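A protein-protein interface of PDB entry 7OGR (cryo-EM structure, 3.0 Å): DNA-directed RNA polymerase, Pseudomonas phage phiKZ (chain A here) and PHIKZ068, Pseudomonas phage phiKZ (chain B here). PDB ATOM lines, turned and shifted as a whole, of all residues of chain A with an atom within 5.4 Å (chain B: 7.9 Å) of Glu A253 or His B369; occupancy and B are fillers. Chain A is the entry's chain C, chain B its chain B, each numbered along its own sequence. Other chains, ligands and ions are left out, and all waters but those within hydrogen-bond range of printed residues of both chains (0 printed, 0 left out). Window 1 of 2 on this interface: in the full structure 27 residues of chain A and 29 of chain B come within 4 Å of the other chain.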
ATOM      1  N   ARG A 243      -1.030 -21.438   7.145  1.00  0.00           N
ATOM      2  CA  ARG A 243      -1.954 -20.360   6.815  1.00  0.00           C
ATOM      3  C   ARG A 243      -1.165 -19.124   6.403  1.00  0.00           C
ATOM      4  O   ARG A 243      -0.128 -18.816   6.995  1.00  0.00           O
ATOM      5  CB  ARG A 243      -2.876 -20.027   7.997  1.00  0.00           C
ATOM      6  CG  ARG A 243      -4.108 -19.213   7.619  1.00  0.00           C
ATOM      7  CD  ARG A 243      -4.787 -18.609   8.839  1.00  0.00           C
ATOM      8  NE  ARG A 243      -4.943 -19.576   9.922  1.00  0.00           N
ATOM      9  CZ  ARG A 243      -6.009 -20.353  10.082  1.00  0.00           C
ATOM     10  NH1 ARG A 243      -6.065 -21.203  11.097  1.00  0.00           N
ATOM     11  NH2 ARG A 243      -7.019 -20.280   9.228  1.00  0.00           N
ATOM     12  N   ASP A 246      -1.992 -12.412   6.535  1.00  0.00           N
ATOM     13  CA  ASP A 246      -2.984 -11.364   6.343  1.00  0.00           C
ATOM     14  C   ASP A 246      -3.175 -10.639   7.665  1.00  0.00           C
ATOM     15  O   ASP A 246      -3.497 -11.271   8.676  1.00  0.00           O
ATOM     16  CB  ASP A 246      -4.317 -11.932   5.844  1.00  0.00           C
ATOM     17  CG  ASP A 246      -4.967 -11.053   4.794  1.00  0.00           C
ATOM     18  OD1 ASP A 246      -4.866  -9.813   4.911  1.00  0.00           O
ATOM     19  OD2 ASP A 246      -5.579 -11.600   3.853  1.00  0.00           O
ATOM     20  N   LEU A 249      -7.187  -9.713   8.519  1.00  0.00           N
ATOM     21  CA  LEU A 249      -7.952 -10.841   9.034  1.00  0.00           C
ATOM     22  C   LEU A 249      -7.422 -11.344  10.372  1.00  0.00           C
ATOM     23  O   LEU A 249      -7.702 -12.487  10.749  1.00  0.00           O
ATOM     24  CB  LEU A 249      -7.958 -11.983   8.014  1.00  0.00           C
ATOM     25  CG  LEU A 249      -8.227 -11.634   6.548  1.00  0.00           C
ATOM     26  CD1 LEU A 249      -8.187 -12.887   5.690  1.00  0.00           C
ATOM     27  CD2 LEU A 249      -9.564 -10.930   6.395  1.00  0.00           C
ATOM     28  N   ALA A 250      -6.664 -10.520  11.093  1.00  0.00           N
ATOM     29  CA  ALA A 250      -6.019 -10.929  12.337  1.00  0.00           C
ATOM     30  C   ALA A 250      -6.971 -11.113  13.527  1.00  0.00           C
ATOM     31  O   ALA A 250      -6.723 -12.018  14.333  1.00  0.00           O
ATOM     32  CB  ALA A 250      -4.893  -9.950  12.693  1.00  0.00           C
ATOM     33  N   PRO A 251      -8.045 -10.320  13.719  1.00  0.00           N
ATOM     34  CA  PRO A 251      -9.056 -10.749  14.703  1.00  0.00           C
ATOM     35  C   PRO A 251      -9.846 -11.972  14.271  1.00  0.00           C
ATOM     36  O   PRO A 251     -10.416 -12.653  15.132  1.00  0.00           O
ATOM     37  CB  PRO A 251      -9.970  -9.523  14.848  1.00  0.00           C
ATOM     38  CG  PRO A 251      -9.688  -8.681  13.686  1.00  0.00           C
ATOM     39  CD  PRO A 251      -8.256  -8.896  13.379  1.00  0.00           C
ATOM     40  N   ALA A 252      -9.900 -12.272  12.973  1.00  0.00           N
ATOM     41  CA  ALA A 252     -10.624 -13.450  12.510  1.00  0.00           C
ATOM     42  C   ALA A 252      -9.755 -14.701  12.567  1.00  0.00           C
ATOM     43  O   ALA A 252     -10.154 -15.715  13.149  1.00  0.00           O
ATOM     44  CB  ALA A 252     -11.138 -13.222  11.089  1.00  0.00           C
ATOM     45  N   GLU A 253      -8.558 -14.643  11.983  1.00  0.00           N
ATOM     46  CA  GLU A 253      -7.737 -15.830  11.788  1.00  0.00           C
ATOM     47  C   GLU A 253      -6.578 -15.960  12.763  1.00  0.00           C
ATOM     48  O   GLU A 253      -6.161 -17.083  13.052  1.00  0.00           O
ATOM     49  CB  GLU A 253      -7.182 -15.859  10.358  1.00  0.00           C
ATOM     50  CG  GLU A 253      -8.246 -15.719   9.285  1.00  0.00           C
ATOM     51  CD  GLU A 253      -7.921 -16.509   8.035  1.00  0.00           C
ATOM     52  OE1 GLU A 253      -7.230 -15.963   7.149  1.00  0.00           O
ATOM     53  OE2 GLU A 253      -8.356 -17.676   7.937  1.00  0.00           O
ATOM     54  N   MET A 254      -6.042 -14.853  13.275  1.00  0.00           N
ATOM     55  CA  MET A 254      -4.947 -14.912  14.245  1.00  0.00           C
ATOM     56  C   MET A 254      -5.496 -14.853  15.672  1.00  0.00           C
ATOM     57  O   MET A 254      -5.202 -13.959  16.465  1.00  0.00           O
ATOM     58  CB  MET A 254      -3.939 -13.801  13.977  1.00  0.00           C
ATOM     59  CG  MET A 254      -3.181 -13.979  12.673  1.00  0.00           C
ATOM     60  SD  MET A 254      -2.018 -12.650  12.342  1.00  0.00           S
ATOM     61  CE  MET A 254      -0.769 -12.986  13.582  1.00  0.00           C
ATOM     62  N   THR A 255      -6.318 -15.853  15.979  1.00  0.00           N
ATOM     63  CA  THR A 255      -6.990 -16.041  17.249  1.00  0.00           C
ATOM     64  C   THR A 255      -6.641 -17.434  17.757  1.00  0.00           C
ATOM     65  O   THR A 255      -6.498 -18.356  16.943  1.00  0.00           O
ATOM     66  CB  THR A 255      -8.513 -15.888  17.066  1.00  0.00           C
ATOM     67  OG1 THR A 255      -8.784 -14.687  16.333  1.00  0.00           O
ATOM     68  CG2 THR A 255      -9.239 -15.806  18.395  1.00  0.00           C
ATOM     69  N   ARG A 257      -8.473 -19.626  18.987  1.00  0.00           N
ATOM     70  CA  ARG A 257      -9.439 -20.588  18.471  1.00  0.00           C
ATOM     71  C   ARG A 257      -9.164 -20.903  17.004  1.00  0.00           C
ATOM     72  O   ARG A 257      -9.196 -22.071  16.601  1.00  0.00           O
ATOM     73  CB  ARG A 257     -10.862 -20.049  18.654  1.00  0.00           C
ATOM     74  CG  ARG A 257     -11.992 -21.071  18.506  1.00  0.00           C
ATOM     75  CD  ARG A 257     -12.611 -21.046  17.114  1.00  0.00           C
ATOM     76  NE  ARG A 257     -12.977 -19.694  16.704  1.00  0.00           N
ATOM     77  CZ  ARG A 257     -13.153 -19.321  15.441  1.00  0.00           C
ATOM     78  NH1 ARG A 257     -13.483 -18.068  15.158  1.00  0.00           N
ATOM     79  NH2 ARG A 257     -12.995 -20.199  14.461  1.00  0.00           N
ATOM     80  N   ALA A 258      -8.891 -19.876  16.197  1.00  0.00           N
ATOM     81  CA  ALA A 258      -8.679 -20.061  14.767  1.00  0.00           C
ATOM     82  C   ALA A 258      -7.295 -20.598  14.430  1.00  0.00           C
ATOM     83  O   ALA A 258      -7.100 -21.096  13.316  1.00  0.00           O
ATOM     84  CB  ALA A 258      -8.910 -18.742  14.027  1.00  0.00           C
ATOM     85  N   LEU A 259      -6.335 -20.510  15.349  1.00  0.00           N
ATOM     86  CA  LEU A 259      -5.021 -21.097  15.124  1.00  0.00           C
ATOM     87  C   LEU A 259      -4.961 -22.565  15.513  1.00  0.00           C
ATOM     88  O   LEU A 259      -4.120 -23.299  14.985  1.00  0.00           O
ATOM     89  CB  LEU A 259      -3.948 -20.321  15.895  1.00  0.00           C
ATOM     90  CG  LEU A 259      -3.614 -18.914  15.391  1.00  0.00           C
ATOM     91  CD1 LEU A 259      -2.634 -18.227  16.328  1.00  0.00           C
ATOM     92  CD2 LEU A 259      -3.062 -18.963  13.976  1.00  0.00           C
ATOM     93  N   ILE B 332     -22.991 -19.110  16.592  1.00  0.00           N
ATOM     94  CA  ILE B 332     -22.105 -18.275  17.397  1.00  0.00           C
ATOM     95  C   ILE B 332     -22.721 -17.957  18.750  1.00  0.00           C
ATOM     96  O   ILE B 332     -22.105 -18.178  19.796  1.00  0.00           O
ATOM     97  CB  ILE B 332     -21.769 -16.989  16.619  1.00  0.00           C
ATOM     98  CG1 ILE B 332     -21.278 -17.340  15.220  1.00  0.00           C
ATOM     99  CG2 ILE B 332     -20.731 -16.171  17.368  1.00  0.00           C
ATOM    100  CD1 ILE B 332     -21.503 -16.248  14.234  1.00  0.00           C
ATOM    101  N   LEU B 363     -15.809  -6.056   8.394  1.00  0.00           N
ATOM    102  CA  LEU B 363     -16.589  -6.253   9.611  1.00  0.00           C
ATOM    103  C   LEU B 363     -17.397  -7.547   9.565  1.00  0.00           C
ATOM    104  O   LEU B 363     -17.710  -8.114  10.618  1.00  0.00           O
ATOM    105  CB  LEU B 363     -17.507  -5.054   9.846  1.00  0.00           C
ATOM    106  CG  LEU B 363     -16.811  -3.782  10.335  1.00  0.00           C
ATOM    107  CD1 LEU B 363     -17.680  -2.559  10.084  1.00  0.00           C
ATOM    108  CD2 LEU B 363     -16.450  -3.896  11.808  1.00  0.00           C
ATOM    109  N   ALA B 364     -17.742  -8.031   8.369  1.00  0.00           N
ATOM    110  CA  ALA B 364     -18.390  -9.329   8.245  1.00  0.00           C
ATOM    111  C   ALA B 364     -17.395 -10.483   8.217  1.00  0.00           C
ATOM    112  O   ALA B 364     -17.804 -11.638   8.367  1.00  0.00           O
ATOM    113  CB  ALA B 364     -19.255  -9.371   6.985  1.00  0.00           C
ATOM    114  N   GLN B 365     -16.112 -10.200   7.992  1.00  0.00           N
ATOM    115  CA  GLN B 365     -15.075 -11.216   8.091  1.00  0.00           C
ATOM    116  C   GLN B 365     -14.551 -11.390   9.508  1.00  0.00           C
ATOM    117  O   GLN B 365     -14.152 -12.502   9.873  1.00  0.00           O
ATOM    118  CB  GLN B 365     -13.908 -10.877   7.160  1.00  0.00           C
ATOM    119  CG  GLN B 365     -14.066 -11.385   5.738  1.00  0.00           C
ATOM    120  CD  GLN B 365     -13.077 -10.746   4.785  1.00  0.00           C
ATOM    121  OE1 GLN B 365     -12.426  -9.759   5.122  1.00  0.00           O
ATOM    122  NE2 GLN B 365     -12.955 -11.310   3.591  1.00  0.00           N
ATOM    123  N   TRP B 366     -14.528 -10.320  10.312  1.00  0.00           N
ATOM    124  CA  TRP B 366     -14.112 -10.461  11.707  1.00  0.00           C
ATOM    125  C   TRP B 366     -15.142 -11.250  12.505  1.00  0.00           C
ATOM    126  O   TRP B 366     -14.807 -12.230  13.182  1.00  0.00           O
ATOM    127  CB  TRP B 366     -13.894  -9.091  12.348  1.00  0.00           C
ATOM    128  CG  TRP B 366     -12.781  -8.285  11.766  1.00  0.00           C
ATOM    129  CD1 TRP B 366     -11.840  -8.699  10.867  1.00  0.00           C
ATOM    130  CD2 TRP B 366     -12.473  -6.924  12.072  1.00  0.00           C
ATOM    131  NE1 TRP B 366     -10.976  -7.670  10.582  1.00  0.00           N
ATOM    132  CE2 TRP B 366     -11.342  -6.569  11.312  1.00  0.00           C
ATOM    133  CE3 TRP B 366     -13.049  -5.966  12.912  1.00  0.00           C
ATOM    134  CZ2 TRP B 366     -10.780  -5.300  11.365  1.00  0.00           C
ATOM    135  CZ3 TRP B 366     -12.487  -4.709  12.964  1.00  0.00           C
ATOM    136  CH2 TRP B 366     -11.362  -4.387  12.199  1.00  0.00           C
ATOM    137  N   VAL B 367     -16.405 -10.833  12.434  1.00  0.00           N
ATOM    138  CA  VAL B 367     -17.525 -11.556  13.023  1.00  0.00           C
ATOM    139  C   VAL B 367     -17.762 -12.766  12.119  1.00  0.00           C
ATOM    140  O   VAL B 367     -17.333 -12.760  10.960  1.00  0.00           O
ATOM    141  CB  VAL B 367     -18.751 -10.618  13.142  1.00  0.00           C
ATOM    142  CG1 VAL B 367     -19.909 -11.220  13.953  1.00  0.00           C
ATOM    143  CG2 VAL B 367     -18.334  -9.281  13.736  1.00  0.00           C
ATOM    144  N   MET B 368     -18.434 -13.799  12.649  1.00  0.00           N
ATOM    145  CA  MET B 368     -18.757 -15.091  12.005  1.00  0.00           C
ATOM    146  C   MET B 368     -17.570 -15.715  11.269  1.00  0.00           C
ATOM    147  O   MET B 368     -17.665 -16.153  10.121  1.00  0.00           O
ATOM    148  CB  MET B 368     -20.007 -15.011  11.100  1.00  0.00           C
ATOM    149  CG  MET B 368     -20.103 -13.993   9.964  1.00  0.00           C
ATOM    150  SD  MET B 368     -21.806 -13.842   9.406  1.00  0.00           S
ATOM    151  CE  MET B 368     -22.618 -13.571  10.977  1.00  0.00           C
ATOM    152  N   HIS B 369     -16.434 -15.762  11.962  1.00  0.00           N
ATOM    153  CA  HIS B 369     -15.368 -16.678  11.586  1.00  0.00           C
ATOM    154  C   HIS B 369     -15.526 -18.036  12.257  1.00  0.00           C
ATOM    155  O   HIS B 369     -14.983 -19.030  11.763  1.00  0.00           O
ATOM    156  CB  HIS B 369     -13.997 -16.086  11.931  1.00  0.00           C
ATOM    157  CG  HIS B 369     -12.848 -16.847  11.347  1.00  0.00           C
ATOM    158  ND1 HIS B 369     -12.385 -16.631  10.067  1.00  0.00           N
ATOM    159  CD2 HIS B 369     -12.077 -17.834  11.863  1.00  0.00           C
ATOM    160  CE1 HIS B 369     -11.375 -17.446   9.822  1.00  0.00           C
ATOM    161  NE2 HIS B 369     -11.167 -18.186  10.896  1.00  0.00           N
ATOM    162  N   LYS B 370     -16.285 -18.096  13.353  1.00  0.00           N
ATOM    163  CA  LYS B 370     -16.514 -19.344  14.070  1.00  0.00           C
ATOM    164  C   LYS B 370     -17.403 -20.309  13.294  1.00  0.00           C
ATOM    165  O   LYS B 370     -17.367 -21.515  13.561  1.00  0.00           O
ATOM    166  CB  LYS B 370     -17.136 -19.038  15.434  1.00  0.00           C
ATOM    167  CG  LYS B 370     -16.893 -20.082  16.507  1.00  0.00           C
ATOM    168  CD  LYS B 370     -17.526 -19.656  17.824  1.00  0.00           C
ATOM    169  CE  LYS B 370     -17.767 -20.844  18.738  1.00  0.00           C
ATOM    170  NZ  LYS B 370     -18.633 -20.479  19.893  1.00  0.00           N
ATOM    171  N   ALA B 371     -18.191 -19.813  12.340  1.00  0.00           N
ATOM    172  CA  ALA B 371     -19.085 -20.657  11.562  1.00  0.00           C
ATOM    173  C   ALA B 371     -18.916 -20.525  10.055  1.00  0.00           C
ATOM    174  O   ALA B 371     -19.483 -21.342   9.322  1.00  0.00           O
ATOM    175  CB  ALA B 371     -20.549 -20.362  11.923  1.00  0.00           C
ATOM    176  N   PHE B 372     -18.161 -19.537   9.568  1.00  0.00           N
ATOM    177  CA  PHE B 372     -17.990 -19.313   8.140  1.00  0.00           C
ATOM    178  C   PHE B 372     -16.547 -18.878   7.898  1.00  0.00           C
ATOM    179  O   PHE B 372     -16.026 -18.038   8.650  1.00  0.00           O
ATOM    180  CB  PHE B 372     -18.970 -18.253   7.627  1.00  0.00           C
ATOM    181  CG  PHE B 372     -19.119 -18.233   6.132  1.00  0.00           C
ATOM    182  CD1 PHE B 372     -20.022 -19.076   5.501  1.00  0.00           C
ATOM    183  CD2 PHE B 372     -18.371 -17.359   5.359  1.00  0.00           C
ATOM    184  CE1 PHE B 372     -20.166 -19.057   4.124  1.00  0.00           C
ATOM    185  CE2 PHE B 372     -18.509 -17.334   3.981  1.00  0.00           C
ATOM    186  CZ  PHE B 372     -19.408 -18.184   3.364  1.00  0.00           C
ATOM    187  N   PRO B 373     -15.872 -19.430   6.888  1.00  0.00           N
ATOM    188  CA  PRO B 373     -14.484 -19.023   6.618  1.00  0.00           C
ATOM    189  C   PRO B 373     -14.419 -17.607   6.060  1.00  0.00           C
ATOM    190  O   PRO B 373     -15.154 -17.252   5.137  1.00  0.00           O
ATOM    191  CB  PRO B 373     -14.001 -20.058   5.596  1.00  0.00           C
ATOM    192  CG  PRO B 373     -15.246 -20.577   4.963  1.00  0.00           C
ATOM    193  CD  PRO B 373     -16.301 -20.545   6.026  1.00  0.00           C
ATOM    194  N   ALA B 374     -13.524 -16.797   6.636  1.00  0.00           N
ATOM    195  CA  ALA B 374     -13.434 -15.392   6.250  1.00  0.00           C
ATOM    196  C   ALA B 374     -12.779 -15.214   4.887  1.00  0.00           C
ATOM    197  O   ALA B 374     -13.028 -14.211   4.208  1.00  0.00           O
ATOM    198  CB  ALA B 374     -12.665 -14.604   7.309  1.00  0.00           C
ATOM    199  N   ARG B 375     -11.946 -16.167   4.466  1.00  0.00           N
ATOM    200  CA  ARG B 375     -11.304 -16.084   3.161  1.00  0.00           C
ATOM    201  C   ARG B 375     -12.223 -16.498   2.020  1.00  0.00           C
ATOM    202  O   ARG B 375     -11.847 -16.335   0.855  1.00  0.00           O
ATOM    203  CB  ARG B 375     -10.036 -16.941   3.142  1.00  0.00           C
ATOM    204  CG  ARG B 375      -8.827 -16.250   3.748  1.00  0.00           C
ATOM    205  CD  ARG B 375      -7.547 -17.029   3.497  1.00  0.00           C
ATOM    206  NE  ARG B 375      -6.484 -16.628   4.415  1.00  0.00           N
ATOM    207  CZ  ARG B 375      -5.594 -15.676   4.156  1.00  0.00           C
ATOM    208  NH1 ARG B 375      -5.635 -15.023   3.003  1.00  0.00           N
ATOM    209  NH2 ARG B 375      -4.662 -15.377   5.050  1.00  0.00           N
ATOM    210  N   ALA B 376     -13.411 -17.024   2.323  1.00  0.00           N
ATOM    211  CA  ALA B 376     -14.380 -17.387   1.300  1.00  0.00           C
ATOM    212  C   ALA B 376     -15.182 -16.200   0.784  1.00  0.00           C
ATOM    213  O   ALA B 376     -15.964 -16.371  -0.154  1.00  0.00           O
ATOM    214  CB  ALA B 376     -15.339 -18.452   1.837  1.00  0.00           C
ATOM    215  N   PHE B 377     -15.009 -15.011   1.372  1.00  0.00           N
ATOM    216  CA  PHE B 377     -15.777 -13.840   0.965  1.00  0.00           C
ATOM    217  C   PHE B 377     -15.394 -13.337  -0.421  1.00  0.00           C
ATOM    218  O   PHE B 377     -16.217 -12.695  -1.082  1.00  0.00           O
ATOM    219  CB  PHE B 377     -15.598 -12.711   1.980  1.00  0.00           C
ATOM    220  CG  PHE B 377     -16.574 -12.752   3.120  1.00  0.00           C
ATOM    221  CD1 PHE B 377     -16.545 -13.790   4.039  1.00  0.00           C
ATOM    222  CD2 PHE B 377     -17.515 -11.746   3.279  1.00  0.00           C
ATOM    223  CE1 PHE B 377     -17.440 -13.829   5.093  1.00  0.00           C
ATOM    224  CE2 PHE B 377     -18.414 -11.777   4.330  1.00  0.00           C
ATOM    225  CZ  PHE B 377     -18.374 -12.819   5.239  1.00  0.00           C
ATOM    226  N   LEU B 395     -25.888  -9.767  14.953  1.00  0.00           N
ATOM    227  CA  LEU B 395     -25.007  -9.990  16.099  1.00  0.00           C
ATOM    228  C   LEU B 395     -24.444  -8.682  16.635  1.00  0.00           C
ATOM    229  O   LEU B 395     -24.303  -8.518  17.853  1.00  0.00           O
ATOM    230  CB  LEU B 395     -23.861 -10.933  15.734  1.00  0.00           C
ATOM    231  CG  LEU B 395     -24.068 -12.447  15.818  1.00  0.00           C
ATOM    232  CD1 LEU B 395     -24.869 -12.971  14.651  1.00  0.00           C
ATOM    233  CD2 LEU B 395     -22.729 -13.150  15.912  1.00  0.00           C
ATOM    234  N   TYR B 442      -4.704 -11.161  21.998  1.00  0.00           N
ATOM    235  CA  TYR B 442      -3.943 -11.404  20.774  1.00  0.00           C
ATOM    236  C   TYR B 442      -2.462 -11.349  21.130  1.00  0.00           C
ATOM    237  O   TYR B 442      -1.819 -10.298  20.987  1.00  0.00           O
ATOM    238  CB  TYR B 442      -4.295 -10.389  19.688  1.00  0.00           C
ATOM    239  CG  TYR B 442      -5.761 -10.374  19.316  1.00  0.00           C
ATOM    240  CD1 TYR B 442      -6.270 -11.266  18.379  1.00  0.00           C
ATOM    241  CD2 TYR B 442      -6.635  -9.463  19.900  1.00  0.00           C
ATOM    242  CE1 TYR B 442      -7.610 -11.254  18.036  1.00  0.00           C
ATOM    243  CE2 TYR B 442      -7.977  -9.443  19.563  1.00  0.00           C
ATOM    244  CZ  TYR B 442      -8.458 -10.341  18.631  1.00  0.00           C
ATOM    245  OH  TYR B 442      -9.791 -10.325  18.292  1.00  0.00           O
ATOM    246  N   HIS B 444       0.234 -12.949  19.825  1.00  0.00           N
ATOM    247  CA  HIS B 444       1.168 -12.970  18.707  1.00  0.00           C
ATOM    248  C   HIS B 444       1.215 -11.593  18.056  1.00  0.00           C
ATOM    249  O   HIS B 444       0.193 -11.092  17.574  1.00  0.00           O
ATOM    250  CB  HIS B 444       0.762 -14.040  17.697  1.00  0.00           C
ATOM    251  CG  HIS B 444       0.443 -15.363  18.320  1.00  0.00           C
ATOM    252  ND1 HIS B 444       1.416 -16.215  18.795  1.00  0.00           N
ATOM    253  CD2 HIS B 444      -0.740 -15.978  18.553  1.00  0.00           C
ATOM    254  CE1 HIS B 444       0.847 -17.299  19.291  1.00  0.00           C
ATOM    255  NE2 HIS B 444      -0.462 -17.180  19.156  1.00  0.00           N
ATOM    256  N   LEU B 516     -14.883  -9.988  20.458  1.00  0.00           N
ATOM    257  CA  LEU B 516     -14.634 -11.143  19.600  1.00  0.00           C
ATOM    258  C   LEU B 516     -13.457 -11.974  20.098  1.00  0.00           C
ATOM    259  O   LEU B 516     -13.437 -13.196  19.909  1.00  0.00           O
ATOM    260  CB  LEU B 516     -14.386 -10.691  18.160  1.00  0.00           C
ATOM    261  CG  LEU B 516     -15.599 -10.206  17.364  1.00  0.00           C
ATOM    262  CD1 LEU B 516     -15.154  -9.471  16.111  1.00  0.00           C
ATOM    263  CD2 LEU B 516     -16.506 -11.372  17.011  1.00  0.00           C
ATOM    264  N   ASN B 520     -13.669 -16.088  21.487  1.00  0.00           N
ATOM    265  CA  ASN B 520     -12.891 -17.153  20.867  1.00  0.00           C
ATOM    266  C   ASN B 520     -11.558 -17.378  21.577  1.00  0.00           C
ATOM    267  O   ASN B 520     -10.547 -17.669  20.933  1.00  0.00           O
ATOM    268  CB  ASN B 520     -12.660 -16.848  19.388  1.00  0.00           C
ATOM    269  CG  ASN B 520     -13.954 -16.724  18.609  1.00  0.00           C
ATOM    270  OD1 ASN B 520     -14.805 -17.612  18.650  1.00  0.00           O
ATOM    271  ND2 ASN B 520     -14.107 -15.619  17.891  1.00  0.00           N
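The guanidinium group (NE) of Arg B375 lies within salt-bridge range of the side-chain carboxylate (OE1) of Glu A253 (2.9 Å).
The guanidinium group (NH1) of Arg A257 lies close to the backbone NH (N) of Lys B370 (3.3 Å).
The backbone carbonyl oxygen of Ala A252 sits close to a ring nitrogen (NE2) of His B369 (3.5 Å).
The side-chain amide oxygen (OD1) of Asn B520 sits at hydrogen-bond distance from the guanidinium group (NE) of Arg A257 (3.4 Å).
The guanidinium group of Arg B375 is in salt-bridge range of the side-chain carboxylate of Asp A246 (3.5 Å).
The side-chain amide nitrogen (NE2) of Gln B365 lies within hydrogen-bond range of the backbone carbonyl oxygen (O) of Ala B374.
The side-chain amide nitrogen (ND2) of Asn B520 is in hydrogen-bond range of the backbone carbonyl oxygen (O) of Leu B516 (3.2 Å).
The guanidinium group (NH1) of Arg A243 is in hydrogen-bond range of the backbone carbonyl oxygen (O) of Ala A258 (2.5 Å).
The backbone carbonyl oxygen of Pro A251 sits at hydrogen-bond distance from the side-chain hydroxyl of Thr A255, at 2.9 Å.
The side-chain carboxylate of Glu A253 lies within salt-bridge range of the guanidinium group of Arg A243 (3.2 Å).
Gln B365 touches Leu A249.
Leu A249 touches Arg B375.
CE1 of Tyr B442 touches O of Ala A250, at 3.9 Å.
Pro A251 touches Trp B366 (CG to NE1, 3.5 Å).
Tyr B442 touches Pro A251.
Gln B365 touches Ala A252 (O to CB, 3.3 Å).
Met A254 touches Tyr B442 (O to CD1, 3.5 Å).
CG2 of Thr A255 touches O of Asn B520, at 3.4 Å.
His B369 touches Ala A258.
His B444 touches Leu A259 (CD2 to CD1, 3.7 Å).
Of the printed residues of chain B, Leu A249 touches Gln B365 (3.3 Å) and Arg B375 (3.9 Å).
Of the printed residues of chain B, Pro A251 touches Trp B366 and Tyr B442.
Of chain B, only His B369 (3.6 Å) and Arg B375 (2.9 Å) come within 4 Å of Glu A253.
His B369 touches four residues of chain A.
Pro B373 touches none of the printed residues of chain A.
Ala B374 touches none of the printed residues of chain A.
The nearest residue of chain A that does not touch His B369 is Arg A243 (4.9 Å).
The nearest printed residue of chain A that does not touch His B444 is Met A254 (4.5 Å).
Of the 21 printed residues of chain B, 8 touch a printed residue of chain A.
Hydrophobic or aromatic side chains of chain B that line the printed part of chain A: Trp B366, His B369, Tyr B442 and His B444.
Among the printed residues, 17 pairs touch across the chains.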
